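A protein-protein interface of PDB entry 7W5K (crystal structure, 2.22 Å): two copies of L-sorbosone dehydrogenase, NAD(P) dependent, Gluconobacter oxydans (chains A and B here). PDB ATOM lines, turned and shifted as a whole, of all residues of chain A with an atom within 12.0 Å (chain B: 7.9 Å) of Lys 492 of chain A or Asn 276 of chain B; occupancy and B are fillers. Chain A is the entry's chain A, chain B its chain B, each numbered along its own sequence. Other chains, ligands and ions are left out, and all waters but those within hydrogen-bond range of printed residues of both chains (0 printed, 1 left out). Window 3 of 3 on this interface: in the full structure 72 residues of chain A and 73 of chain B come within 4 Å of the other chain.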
ATOM      1  N   GLY A 141     -12.906 -14.283  11.085  1.00  0.00           N
ATOM      2  CA  GLY A 141     -14.257 -14.414  11.594  1.00  0.00           C
ATOM      3  C   GLY A 141     -15.222 -13.483  10.884  1.00  0.00           C
ATOM      4  O   GLY A 141     -14.806 -12.493  10.265  1.00  0.00           O
ATOM      5  N   GLU A 142     -16.524 -13.782  10.979  1.00  0.00           N
ATOM      6  CA  GLU A 142     -17.521 -12.965  10.293  1.00  0.00           C
ATOM      7  C   GLU A 142     -17.462 -11.518  10.748  1.00  0.00           C
ATOM      8  O   GLU A 142     -17.680 -10.606   9.941  1.00  0.00           O
ATOM      9  CB  GLU A 142     -18.938 -13.501  10.521  1.00  0.00           C
ATOM     10  CG  GLU A 142     -19.295 -14.776   9.798  1.00  0.00           C
ATOM     11  CD  GLU A 142     -20.358 -15.551  10.548  1.00  0.00           C
ATOM     12  OE1 GLU A 142     -21.185 -14.902  11.221  1.00  0.00           O
ATOM     13  OE2 GLU A 142     -20.372 -16.797  10.465  1.00  0.00           O
ATOM     14  N   GLY A 143     -17.234 -11.286  12.036  1.00  0.00           N
ATOM     15  CA  GLY A 143     -17.296  -9.951  12.575  1.00  0.00           C
ATOM     16  C   GLY A 143     -15.969  -9.255  12.742  1.00  0.00           C
ATOM     17  O   GLY A 143     -15.934  -8.162  13.318  1.00  0.00           O
ATOM     18  N   LEU A 144     -14.877  -9.836  12.260  1.00  0.00           N
ATOM     19  CA  LEU A 144     -13.568  -9.208  12.404  1.00  0.00           C
ATOM     20  C   LEU A 144     -12.851  -9.323  11.070  1.00  0.00           C
ATOM     21  O   LEU A 144     -12.546 -10.429  10.606  1.00  0.00           O
ATOM     22  CB  LEU A 144     -12.762  -9.841  13.530  1.00  0.00           C
ATOM     23  CG  LEU A 144     -11.388  -9.210  13.760  1.00  0.00           C
ATOM     24  CD1 LEU A 144     -11.516  -7.748  14.179  1.00  0.00           C
ATOM     25  CD2 LEU A 144     -10.620 -10.004  14.799  1.00  0.00           C
ATOM     26  N   PHE A 145     -12.610  -8.183  10.448  1.00  0.00           N
ATOM     27  CA  PHE A 145     -11.858  -8.115   9.211  1.00  0.00           C
ATOM     28  C   PHE A 145     -10.491  -7.535   9.527  1.00  0.00           C
ATOM     29  O   PHE A 145     -10.386  -6.526  10.234  1.00  0.00           O
ATOM     30  CB  PHE A 145     -12.566  -7.256   8.170  1.00  0.00           C
ATOM     31  CG  PHE A 145     -11.858  -7.226   6.867  1.00  0.00           C
ATOM     32  CD1 PHE A 145     -11.826  -8.352   6.069  1.00  0.00           C
ATOM     33  CD2 PHE A 145     -11.183  -6.097   6.454  1.00  0.00           C
ATOM     34  CE1 PHE A 145     -11.156  -8.338   4.867  1.00  0.00           C
ATOM     35  CE2 PHE A 145     -10.521  -6.074   5.247  1.00  0.00           C
ATOM     36  CZ  PHE A 145     -10.500  -7.192   4.459  1.00  0.00           C
ATOM     37  N   ILE A 488     -11.022  -4.353  11.675  1.00  0.00           N
ATOM     38  CA  ILE A 488     -12.348  -3.783  11.582  1.00  0.00           C
ATOM     39  C   ILE A 488     -13.297  -4.797  12.198  1.00  0.00           C
ATOM     40  O   ILE A 488     -13.363  -5.953  11.755  1.00  0.00           O
ATOM     41  CB  ILE A 488     -12.714  -3.489  10.118  1.00  0.00           C
ATOM     42  CG1 ILE A 488     -11.537  -2.778   9.439  1.00  0.00           C
ATOM     43  CG2 ILE A 488     -14.007  -2.703  10.037  1.00  0.00           C
ATOM     44  CD1 ILE A 488     -11.781  -2.375   7.975  1.00  0.00           C
ATOM     45  N   GLU A 489     -14.018  -4.375  13.221  1.00  0.00           N
ATOM     46  CA  GLU A 489     -15.086  -5.185  13.753  1.00  0.00           C
ATOM     47  C   GLU A 489     -16.376  -4.737  13.095  1.00  0.00           C
ATOM     48  O   GLU A 489     -16.678  -3.543  13.070  1.00  0.00           O
ATOM     49  CB  GLU A 489     -15.188  -5.064  15.274  1.00  0.00           C
ATOM     50  CG  GLU A 489     -16.046  -6.157  15.883  1.00  0.00           C
ATOM     51  CD  GLU A 489     -15.656  -6.481  17.307  1.00  0.00           C
ATOM     52  OE1 GLU A 489     -14.589  -6.001  17.763  1.00  0.00           O
ATOM     53  OE2 GLU A 489     -16.431  -7.208  17.970  1.00  0.00           O
ATOM     54  N   THR A 490     -17.098  -5.684  12.515  1.00  0.00           N
ATOM     55  CA  THR A 490     -18.426  -5.432  11.993  1.00  0.00           C
ATOM     56  C   THR A 490     -19.442  -6.013  12.967  1.00  0.00           C
ATOM     57  O   THR A 490     -19.091  -6.613  13.985  1.00  0.00           O
ATOM     58  CB  THR A 490     -18.573  -6.004  10.583  1.00  0.00           C
ATOM     59  OG1 THR A 490     -18.138  -7.373  10.548  1.00  0.00           O
ATOM     60  CG2 THR A 490     -17.721  -5.207   9.635  1.00  0.00           C
ATOM     61  N   GLY A 491     -20.715  -5.810  12.673  1.00  0.00           N
ATOM     62  CA  GLY A 491     -21.672  -6.345  13.622  1.00  0.00           C
ATOM     63  C   GLY A 491     -21.704  -5.537  14.916  1.00  0.00           C
ATOM     64  O   GLY A 491     -21.313  -4.364  14.973  1.00  0.00           O
ATOM     65  N   LYS A 492     -22.177  -6.191  15.975  1.00  0.00           N
ATOM     66  CA  LYS A 492     -22.429  -5.518  17.243  1.00  0.00           C
ATOM     67  C   LYS A 492     -21.267  -5.721  18.207  1.00  0.00           C
ATOM     68  O   LYS A 492     -20.745  -6.834  18.349  1.00  0.00           O
ATOM     69  CB  LYS A 492     -23.733  -6.008  17.883  1.00  0.00           C
ATOM     70  CG  LYS A 492     -24.916  -5.060  17.663  1.00  0.00           C
ATOM     71  CD  LYS A 492     -24.609  -3.646  18.186  1.00  0.00           C
ATOM     72  CE  LYS A 492     -25.800  -2.698  17.986  1.00  0.00           C
ATOM     73  NZ  LYS A 492     -25.979  -1.721  19.108  1.00  0.00           N
ATOM     74  N   ARG A 493     -20.862  -4.628  18.860  1.00  0.00           N
ATOM     75  CA  ARG A 493     -19.805  -4.709  19.859  1.00  0.00           C
ATOM     76  C   ARG A 493     -20.340  -5.361  21.123  1.00  0.00           C
ATOM     77  O   ARG A 493     -21.388  -4.960  21.646  1.00  0.00           O
ATOM     78  CB  ARG A 493     -19.244  -3.324  20.186  1.00  0.00           C
ATOM     79  CG  ARG A 493     -18.275  -3.352  21.384  1.00  0.00           C
ATOM     80  CD  ARG A 493     -17.539  -2.026  21.649  1.00  0.00           C
ATOM     81  NE  ARG A 493     -16.684  -2.131  22.834  1.00  0.00           N
ATOM     82  CZ  ARG A 493     -15.445  -2.621  22.830  1.00  0.00           C
ATOM     83  NH1 ARG A 493     -14.857  -3.007  21.707  1.00  0.00           N
ATOM     84  NH2 ARG A 493     -14.784  -2.741  23.981  1.00  0.00           N
ATOM     85  N   SER A 494     -19.634  -6.379  21.603  1.00  0.00           N
ATOM     86  CA  SER A 494     -19.909  -6.923  22.926  1.00  0.00           C
ATOM     87  C   SER A 494     -19.234  -6.013  23.945  1.00  0.00           C
ATOM     88  O   SER A 494     -18.008  -5.872  23.949  1.00  0.00           O
ATOM     89  CB  SER A 494     -19.407  -8.361  23.041  1.00  0.00           C
ATOM     90  OG  SER A 494     -19.322  -8.747  24.395  1.00  0.00           O
ATOM     91  N   HIS A 495     -20.027  -5.352  24.771  1.00  0.00           N
ATOM     92  CA  HIS A 495     -19.476  -4.280  25.575  1.00  0.00           C
ATOM     93  C   HIS A 495     -18.607  -4.834  26.695  1.00  0.00           C
ATOM     94  O   HIS A 495     -18.923  -5.852  27.313  1.00  0.00           O
ATOM     95  CB  HIS A 495     -20.597  -3.412  26.136  1.00  0.00           C
ATOM     96  CG  HIS A 495     -21.088  -2.389  25.168  1.00  0.00           C
ATOM     97  ND1 HIS A 495     -21.613  -1.180  25.566  1.00  0.00           N
ATOM     98  CD2 HIS A 495     -21.124  -2.390  23.814  1.00  0.00           C
ATOM     99  CE1 HIS A 495     -21.950  -0.477  24.499  1.00  0.00           C
ATOM    100  NE2 HIS A 495     -21.674  -1.193  23.424  1.00  0.00           N
ATOM    101  N   TRP A 496     -17.497  -4.148  26.943  1.00  0.00           N
ATOM    102  CA  TRP A 496     -16.633  -4.483  28.066  1.00  0.00           C
ATOM    103  C   TRP A 496     -17.309  -4.191  29.396  1.00  0.00           C
ATOM    104  O   TRP A 496     -17.242  -4.999  30.331  1.00  0.00           O
ATOM    105  CB  TRP A 496     -15.344  -3.686  27.954  1.00  0.00           C
ATOM    106  CG  TRP A 496     -14.364  -4.017  28.975  1.00  0.00           C
ATOM    107  CD1 TRP A 496     -13.965  -5.266  29.358  1.00  0.00           C
ATOM    108  CD2 TRP A 496     -13.617  -3.094  29.764  1.00  0.00           C
ATOM    109  NE1 TRP A 496     -13.010  -5.172  30.340  1.00  0.00           N
ATOM    110  CE2 TRP A 496     -12.778  -3.848  30.606  1.00  0.00           C
ATOM    111  CE3 TRP A 496     -13.580  -1.702  29.842  1.00  0.00           C
ATOM    112  CZ2 TRP A 496     -11.906  -3.259  31.507  1.00  0.00           C
ATOM    113  CZ3 TRP A 496     -12.715  -1.114  30.730  1.00  0.00           C
ATOM    114  CH2 TRP A 496     -11.887  -1.892  31.559  1.00  0.00           C
ATOM    115  N   ILE A 497     -17.973  -3.050  29.491  1.00  0.00           N
ATOM    116  CA  ILE A 497     -18.553  -2.571  30.734  1.00  0.00           C
ATOM    117  C   ILE A 497     -20.026  -2.949  30.773  1.00  0.00           C
ATOM    118  O   ILE A 497     -20.763  -2.721  29.802  1.00  0.00           O
ATOM    119  CB  ILE A 497     -18.361  -1.055  30.867  1.00  0.00           C
ATOM    120  CG1 ILE A 497     -16.897  -0.741  31.214  1.00  0.00           C
ATOM    121  CG2 ILE A 497     -19.320  -0.480  31.887  1.00  0.00           C
ATOM    122  CD1 ILE A 497     -16.294   0.371  30.366  1.00  0.00           C
ATOM    123  N   VAL B 271     -13.226   9.354  17.397  1.00  0.00           N
ATOM    124  CA  VAL B 271     -14.638   9.004  17.470  1.00  0.00           C
ATOM    125  C   VAL B 271     -15.425  10.020  16.667  1.00  0.00           C
ATOM    126  O   VAL B 271     -15.404  11.213  16.977  1.00  0.00           O
ATOM    127  CB  VAL B 271     -15.154   8.941  18.910  1.00  0.00           C
ATOM    128  CG1 VAL B 271     -16.663   8.663  18.880  1.00  0.00           C
ATOM    129  CG2 VAL B 271     -14.425   7.845  19.675  1.00  0.00           C
ATOM    130  N   PHE B 272     -16.113   9.548  15.644  1.00  0.00           N
ATOM    131  CA  PHE B 272     -16.982  10.401  14.855  1.00  0.00           C
ATOM    132  C   PHE B 272     -18.402  10.354  15.396  1.00  0.00           C
ATOM    133  O   PHE B 272     -18.839   9.357  15.986  1.00  0.00           O
ATOM    134  CB  PHE B 272     -16.972   9.987  13.389  1.00  0.00           C
ATOM    135  CG  PHE B 272     -15.708  10.342  12.694  1.00  0.00           C
ATOM    136  CD1 PHE B 272     -15.536  11.608  12.147  1.00  0.00           C
ATOM    137  CD2 PHE B 272     -14.662   9.431  12.624  1.00  0.00           C
ATOM    138  CE1 PHE B 272     -14.344  11.956  11.526  1.00  0.00           C
ATOM    139  CE2 PHE B 272     -13.482   9.760  11.996  1.00  0.00           C
ATOM    140  CZ  PHE B 272     -13.310  11.025  11.448  1.00  0.00           C
ATOM    141  N   ALA B 273     -19.125  11.450  15.152  1.00  0.00           N
ATOM    142  CA  ALA B 273     -20.520  11.566  15.559  1.00  0.00           C
ATOM    143  C   ALA B 273     -21.365  10.441  14.996  1.00  0.00           C
ATOM    144  O   ALA B 273     -22.378  10.065  15.595  1.00  0.00           O
ATOM    145  CB  ALA B 273     -21.077  12.915  15.106  1.00  0.00           C
ATOM    146  N   ASP B 274     -21.005   9.925  13.829  1.00  0.00           N
ATOM    147  CA  ASP B 274     -21.771   8.859  13.207  1.00  0.00           C
ATOM    148  C   ASP B 274     -21.310   7.475  13.654  1.00  0.00           C
ATOM    149  O   ASP B 274     -21.688   6.474  13.036  1.00  0.00           O
ATOM    150  CB  ASP B 274     -21.733   8.987  11.679  1.00  0.00           C
ATOM    151  CG  ASP B 274     -20.332   8.865  11.103  1.00  0.00           C
ATOM    152  OD1 ASP B 274     -19.423   8.376  11.812  1.00  0.00           O
ATOM    153  OD2 ASP B 274     -20.154   9.249   9.921  1.00  0.00           O
ATOM    154  N   SER B 275     -20.463   7.399  14.674  1.00  0.00           N
ATOM    155  CA  SER B 275     -20.150   6.101  15.228  1.00  0.00           C
ATOM    156  C   SER B 275     -21.301   5.624  16.104  1.00  0.00           C
ATOM    157  O   SER B 275     -22.201   6.382  16.465  1.00  0.00           O
ATOM    158  CB  SER B 275     -18.851   6.157  16.029  1.00  0.00           C
ATOM    159  OG  SER B 275     -19.015   6.870  17.242  1.00  0.00           O
ATOM    160  N   ASN B 276     -21.284   4.342  16.427  1.00  0.00           N
ATOM    161  CA  ASN B 276     -22.126   3.836  17.503  1.00  0.00           C
ATOM    162  C   ASN B 276     -21.535   4.373  18.797  1.00  0.00           C
ATOM    163  O   ASN B 276     -20.497   3.895  19.272  1.00  0.00           O
ATOM    164  CB  ASN B 276     -22.177   2.312  17.487  1.00  0.00           C
ATOM    165  CG  ASN B 276     -23.193   1.752  18.475  1.00  0.00           C
ATOM    166  OD1 ASN B 276     -23.217   2.124  19.655  1.00  0.00           O
ATOM    167  ND2 ASN B 276     -24.030   0.852  17.995  1.00  0.00           N
ATOM    168  N   LEU B 277     -22.153   5.427  19.324  1.00  0.00           N
ATOM    169  CA  LEU B 277     -21.548   6.166  20.422  1.00  0.00           C
ATOM    170  C   LEU B 277     -21.436   5.298  21.659  1.00  0.00           C
ATOM    171  O   LEU B 277     -20.452   5.383  22.399  1.00  0.00           O
ATOM    172  CB  LEU B 277     -22.372   7.410  20.727  1.00  0.00           C
ATOM    173  CG  LEU B 277     -22.336   8.464  19.641  1.00  0.00           C
ATOM    174  CD1 LEU B 277     -23.148   9.655  20.102  1.00  0.00           C
ATOM    175  CD2 LEU B 277     -20.888   8.859  19.311  1.00  0.00           C
ATOM    176  N   GLU B 278     -22.430   4.449  21.895  1.00  0.00           N
ATOM    177  CA  GLU B 278     -22.360   3.566  23.049  1.00  0.00           C
ATOM    178  C   GLU B 278     -21.202   2.587  22.903  1.00  0.00           C
ATOM    179  O   GLU B 278     -20.410   2.407  23.834  1.00  0.00           O
ATOM    180  CB  GLU B 278     -23.681   2.821  23.207  1.00  0.00           C
ATOM    181  CG  GLU B 278     -24.743   3.569  23.976  1.00  0.00           C
ATOM    182  CD  GLU B 278     -26.038   2.793  24.014  1.00  0.00           C
ATOM    183  OE1 GLU B 278     -25.999   1.578  24.327  1.00  0.00           O
ATOM    184  OE2 GLU B 278     -27.087   3.382  23.691  1.00  0.00           O
ATOM    185  N   ASP B 279     -21.082   1.966  21.725  1.00  0.00           N
ATOM    186  CA  ASP B 279     -19.969   1.059  21.451  1.00  0.00           C
ATOM    187  C   ASP B 279     -18.639   1.777  21.558  1.00  0.00           C
ATOM    188  O   ASP B 279     -17.691   1.262  22.165  1.00  0.00           O
ATOM    189  CB  ASP B 279     -20.128   0.430  20.070  1.00  0.00           C
ATOM    190  CG  ASP B 279     -21.300  -0.525  20.007  1.00  0.00           C
ATOM    191  OD1 ASP B 279     -21.906  -0.758  21.069  1.00  0.00           O
ATOM    192  OD2 ASP B 279     -21.624  -1.025  18.909  1.00  0.00           O
ATOM    193  N   ALA B 280     -18.543   2.963  20.945  1.00  0.00           N
ATOM    194  CA  ALA B 280     -17.295   3.717  20.976  1.00  0.00           C
ATOM    195  C   ALA B 280     -16.934   4.119  22.397  1.00  0.00           C
ATOM    196  O   ALA B 280     -15.768   4.033  22.794  1.00  0.00           O
ATOM    197  CB  ALA B 280     -17.395   4.940  20.064  1.00  0.00           C
ATOM    198  N   ALA B 281     -17.928   4.559  23.180  1.00  0.00           N
ATOM    199  CA  ALA B 281     -17.679   4.937  24.567  1.00  0.00           C
ATOM    200  C   ALA B 281     -17.151   3.756  25.360  1.00  0.00           C
ATOM    201  O   ALA B 281     -16.166   3.874  26.096  1.00  0.00           O
ATOM    202  CB  ALA B 281     -18.959   5.474  25.207  1.00  0.00           C
ATOM    203  N   ASP B 282     -17.783   2.596  25.203  1.00  0.00           N
ATOM    204  CA  ASP B 282     -17.260   1.392  25.838  1.00  0.00           C
ATOM    205  C   ASP B 282     -15.832   1.109  25.381  1.00  0.00           C
ATOM    206  O   ASP B 282     -14.940   0.845  26.198  1.00  0.00           O
ATOM    207  CB  ASP B 282     -18.149   0.207  25.518  1.00  0.00           C
ATOM    208  CG  ASP B 282     -17.691  -1.035  26.220  1.00  0.00           C
ATOM    209  OD1 ASP B 282     -18.025  -1.190  27.414  1.00  0.00           O
ATOM    210  OD2 ASP B 282     -16.979  -1.840  25.586  1.00  0.00           O
ATOM    211  N   ALA B 283     -15.593   1.185  24.074  1.00  0.00           N
ATOM    212  CA  ALA B 283     -14.260   0.920  23.549  1.00  0.00           C
ATOM    213  C   ALA B 283     -13.242   1.945  24.021  1.00  0.00           C
ATOM    214  O   ALA B 283     -12.087   1.602  24.294  1.00  0.00           O
ATOM    215  CB  ALA B 283     -14.307   0.928  22.041  1.00  0.00           C
ATOM    216  N   PHE B 312     -20.125  12.605  24.275  1.00  0.00           N
ATOM    217  CA  PHE B 312     -19.346  11.377  24.206  1.00  0.00           C
ATOM    218  C   PHE B 312     -18.396  11.259  25.384  1.00  0.00           C
ATOM    219  O   PHE B 312     -18.239  10.171  25.941  1.00  0.00           O
ATOM    220  CB  PHE B 312     -18.561  11.291  22.900  1.00  0.00           C
ATOM    221  CG  PHE B 312     -17.857   9.991  22.742  1.00  0.00           C
ATOM    222  CD1 PHE B 312     -18.563   8.857  22.388  1.00  0.00           C
ATOM    223  CD2 PHE B 312     -16.499   9.882  23.012  1.00  0.00           C
ATOM    224  CE1 PHE B 312     -17.927   7.645  22.268  1.00  0.00           C
ATOM    225  CE2 PHE B 312     -15.862   8.663  22.898  1.00  0.00           C
ATOM    226  CZ  PHE B 312     -16.571   7.550  22.523  1.00  0.00           C
ATOM    227  N   LEU B 315     -20.339   9.944  28.028  1.00  0.00           N
ATOM    228  CA  LEU B 315     -20.556   8.514  27.812  1.00  0.00           C
ATOM    229  C   LEU B 315     -19.344   7.718  28.271  1.00  0.00           C
ATOM    230  O   LEU B 315     -19.479   6.624  28.842  1.00  0.00           O
ATOM    231  CB  LEU B 315     -20.861   8.225  26.342  1.00  0.00           C
ATOM    232  CG  LEU B 315     -22.132   8.862  25.798  1.00  0.00           C
ATOM    233  CD1 LEU B 315     -22.357   8.487  24.321  1.00  0.00           C
ATOM    234  CD2 LEU B 315     -23.329   8.487  26.670  1.00  0.00           C
ATOM    235  N   TRP B 427     -13.634   5.331  15.119  1.00  0.00           N
ATOM    236  CA  TRP B 427     -15.005   4.906  15.312  1.00  0.00           C
ATOM    237  C   TRP B 427     -15.869   5.762  14.400  1.00  0.00           C
ATOM    238  O   TRP B 427     -15.934   6.993  14.553  1.00  0.00           O
ATOM    239  CB  TRP B 427     -15.390   5.025  16.778  1.00  0.00           C
ATOM    240  CG  TRP B 427     -14.783   3.928  17.533  1.00  0.00           C
ATOM    241  CD1 TRP B 427     -13.491   3.860  18.001  1.00  0.00           C
ATOM    242  CD2 TRP B 427     -15.403   2.700  17.886  1.00  0.00           C
ATOM    243  NE1 TRP B 427     -13.280   2.656  18.631  1.00  0.00           N
ATOM    244  CE2 TRP B 427     -14.441   1.927  18.579  1.00  0.00           C
ATOM    245  CE3 TRP B 427     -16.686   2.172  17.696  1.00  0.00           C
ATOM    246  CZ2 TRP B 427     -14.723   0.663  19.066  1.00  0.00           C
ATOM    247  CZ3 TRP B 427     -16.962   0.908  18.191  1.00  0.00           C
ATOM    248  CH2 TRP B 427     -15.992   0.172  18.872  1.00  0.00           C
ATOM    249  N   SER B 428     -16.478   5.111  13.420  1.00  0.00           N
ATOM    250  CA  SER B 428     -17.351   5.782  12.476  1.00  0.00           C
ATOM    251  C   SER B 428     -18.057   4.709  11.683  1.00  0.00           C
ATOM    252  O   SER B 428     -17.467   3.668  11.385  1.00  0.00           O
ATOM    253  CB  SER B 428     -16.580   6.724  11.549  1.00  0.00           C
ATOM    254  OG  SER B 428     -17.443   7.215  10.553  1.00  0.00           O
ATOM    255  N   LYS B 429     -19.338   4.928  11.420  1.00  0.00           N
ATOM    256  CA  LYS B 429     -20.018   4.046  10.487  1.00  0.00           C
ATOM    257  C   LYS B 429     -19.717   4.432   9.052  1.00  0.00           C
ATOM    258  O   LYS B 429     -20.035   3.674   8.135  1.00  0.00           O
ATOM    259  CB  LYS B 429     -21.535   4.067  10.730  1.00  0.00           C
ATOM    260  CG  LYS B 429     -22.017   3.450  12.056  1.00  0.00           C
ATOM    261  CD  LYS B 429     -20.998   2.509  12.725  1.00  0.00           C
ATOM    262  CE  LYS B 429     -21.016   1.079  12.165  1.00  0.00           C
ATOM    263  NZ  LYS B 429     -20.353   0.117  13.123  1.00  0.00           N
ATOM    264  N   ASN B 449     -13.807   0.753  14.532  1.00  0.00           N
ATOM    265  CA  ASN B 449     -14.999   0.321  15.262  1.00  0.00           C
ATOM    266  C   ASN B 449     -14.689  -0.867  16.159  1.00  0.00           C
ATOM    267  O   ASN B 449     -15.521  -1.754  16.354  1.00  0.00           O
ATOM    268  CB  ASN B 449     -16.145  -0.003  14.304  1.00  0.00           C
ATOM    269  CG  ASN B 449     -16.530   1.192  13.472  1.00  0.00           C
ATOM    270  OD1 ASN B 449     -16.465   2.332  13.948  1.00  0.00           O
ATOM    271  ND2 ASN B 449     -16.907   0.954  12.220  1.00  0.00           N
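NZ of Lys 492 of chain A sits close to ND2 of Asn 276 of chain B. The guanidinium group (NE) of Arg 493 of chain A is in salt-bridge range of the side-chain carboxylate (OD2) of Asp 282 of chain B, at 2.8 Å. A ring nitrogen (NE2) of His 495 of chain A sits at hydrogen-bond distance from the side-chain carboxylate (OD1) of Asp 279 of chain B, at 2.4 Å. The backbone NH (N) of Trp 496 of chain A sits at hydrogen-bond distance from the side-chain carboxylate (OD2) of Asp 282 of chain B (2.7 Å). The backbone NH of Ile 497 of chain A is in hydrogen-bond range of the side-chain carboxylate of Asp 282 of chain B (2.8 Å).
The backbone carbonyl oxygen of Trp 427 of chain B lies within hydrogen-bond range of the backbone NH of Phe 272 of chain B (2.8 Å). OD1 of Asn 276 of chain B lies close to N of Glu 278 of chain B. The side-chain amide oxygen (OD1) of Asn 276 of chain B lies within hydrogen-bond range of the backbone NH (N) of Asp 279 of chain B (3.0 Å). OD1 of Asn 449 of chain B lies within hydrogen-bond range of N of Ser 428 of chain B (2.8 Å).
Among the printed residues, pairs that only touch across the chains: Glu 489 of chain A with Asn 449 of chain B, Arg 493 of chain A with Asp 279 of chain B, Arg 493 of chain A with Ala 283 of chain B, Arg 493 of chain A with Trp 427 of chain B, His 495 of chain A with Glu 278 of chain B and His 495 of chain A with Asp 282 of chain B.
Of the printed residues of chain B, Glu 489 of chain A touches Asn 449 (3.5 Å). No residue of chain B comes within 4 Å of Gly 491 of chain A. Of chain B, only Asn 276 comes within 4 Å of Lys 492 of chain A. Printed residues of chain B within 4 Å of Arg 493 of chain A: Asp 279, Asp 282, Ala 283 and Trp 427. Printed residues of chain B within 4 Å of His 495 of chain A: Glu 278 (3.3 Å), Asp 279 (2.4 Å) and Asp 282 (3.5 Å). Printed residues of chain B within 4 Å of Ile 497 of chain A: Asp 282. Asn 276 of chain B touches just one residue of chain A: Lys 492 (3.4 Å). No residue of chain A comes within 4 Å of Ala 280 of chain B. Ala 281 of chain B touches none of the printed residues of chain A. Of the printed residues of chain A, Asp 282 of chain B touches Arg 493 (2.8 Å), His 495 (3.5 Å), Trp 496 (2.7 Å) and Ile 497 (2.8 Å). Of the printed residues of chain A, Trp 427 of chain B touches Arg 493 (3.9 Å). No residue of chain A comes within 4 Å of Ser 428 of chain B. The nearest residue of chain B that does not touch Lys 492 of chain A is Asp 279 of chain B (4.04 Å). The nearest residue of chain A that does not touch Asn 276 of chain B is His 495 of chain A (5.3 Å).
Of the 19 printed residues of chain B, 7 touch a printed residue of chain A. Hydrophobic or aromatic side chains of chain B within 4 Å of the printed part of chain A: Ala 283 and Trp 427.
No position is printed for both chains. Of the 11 pairs that touch across the chains among the printed residues, none has its exchanged pair printed and touching as well.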
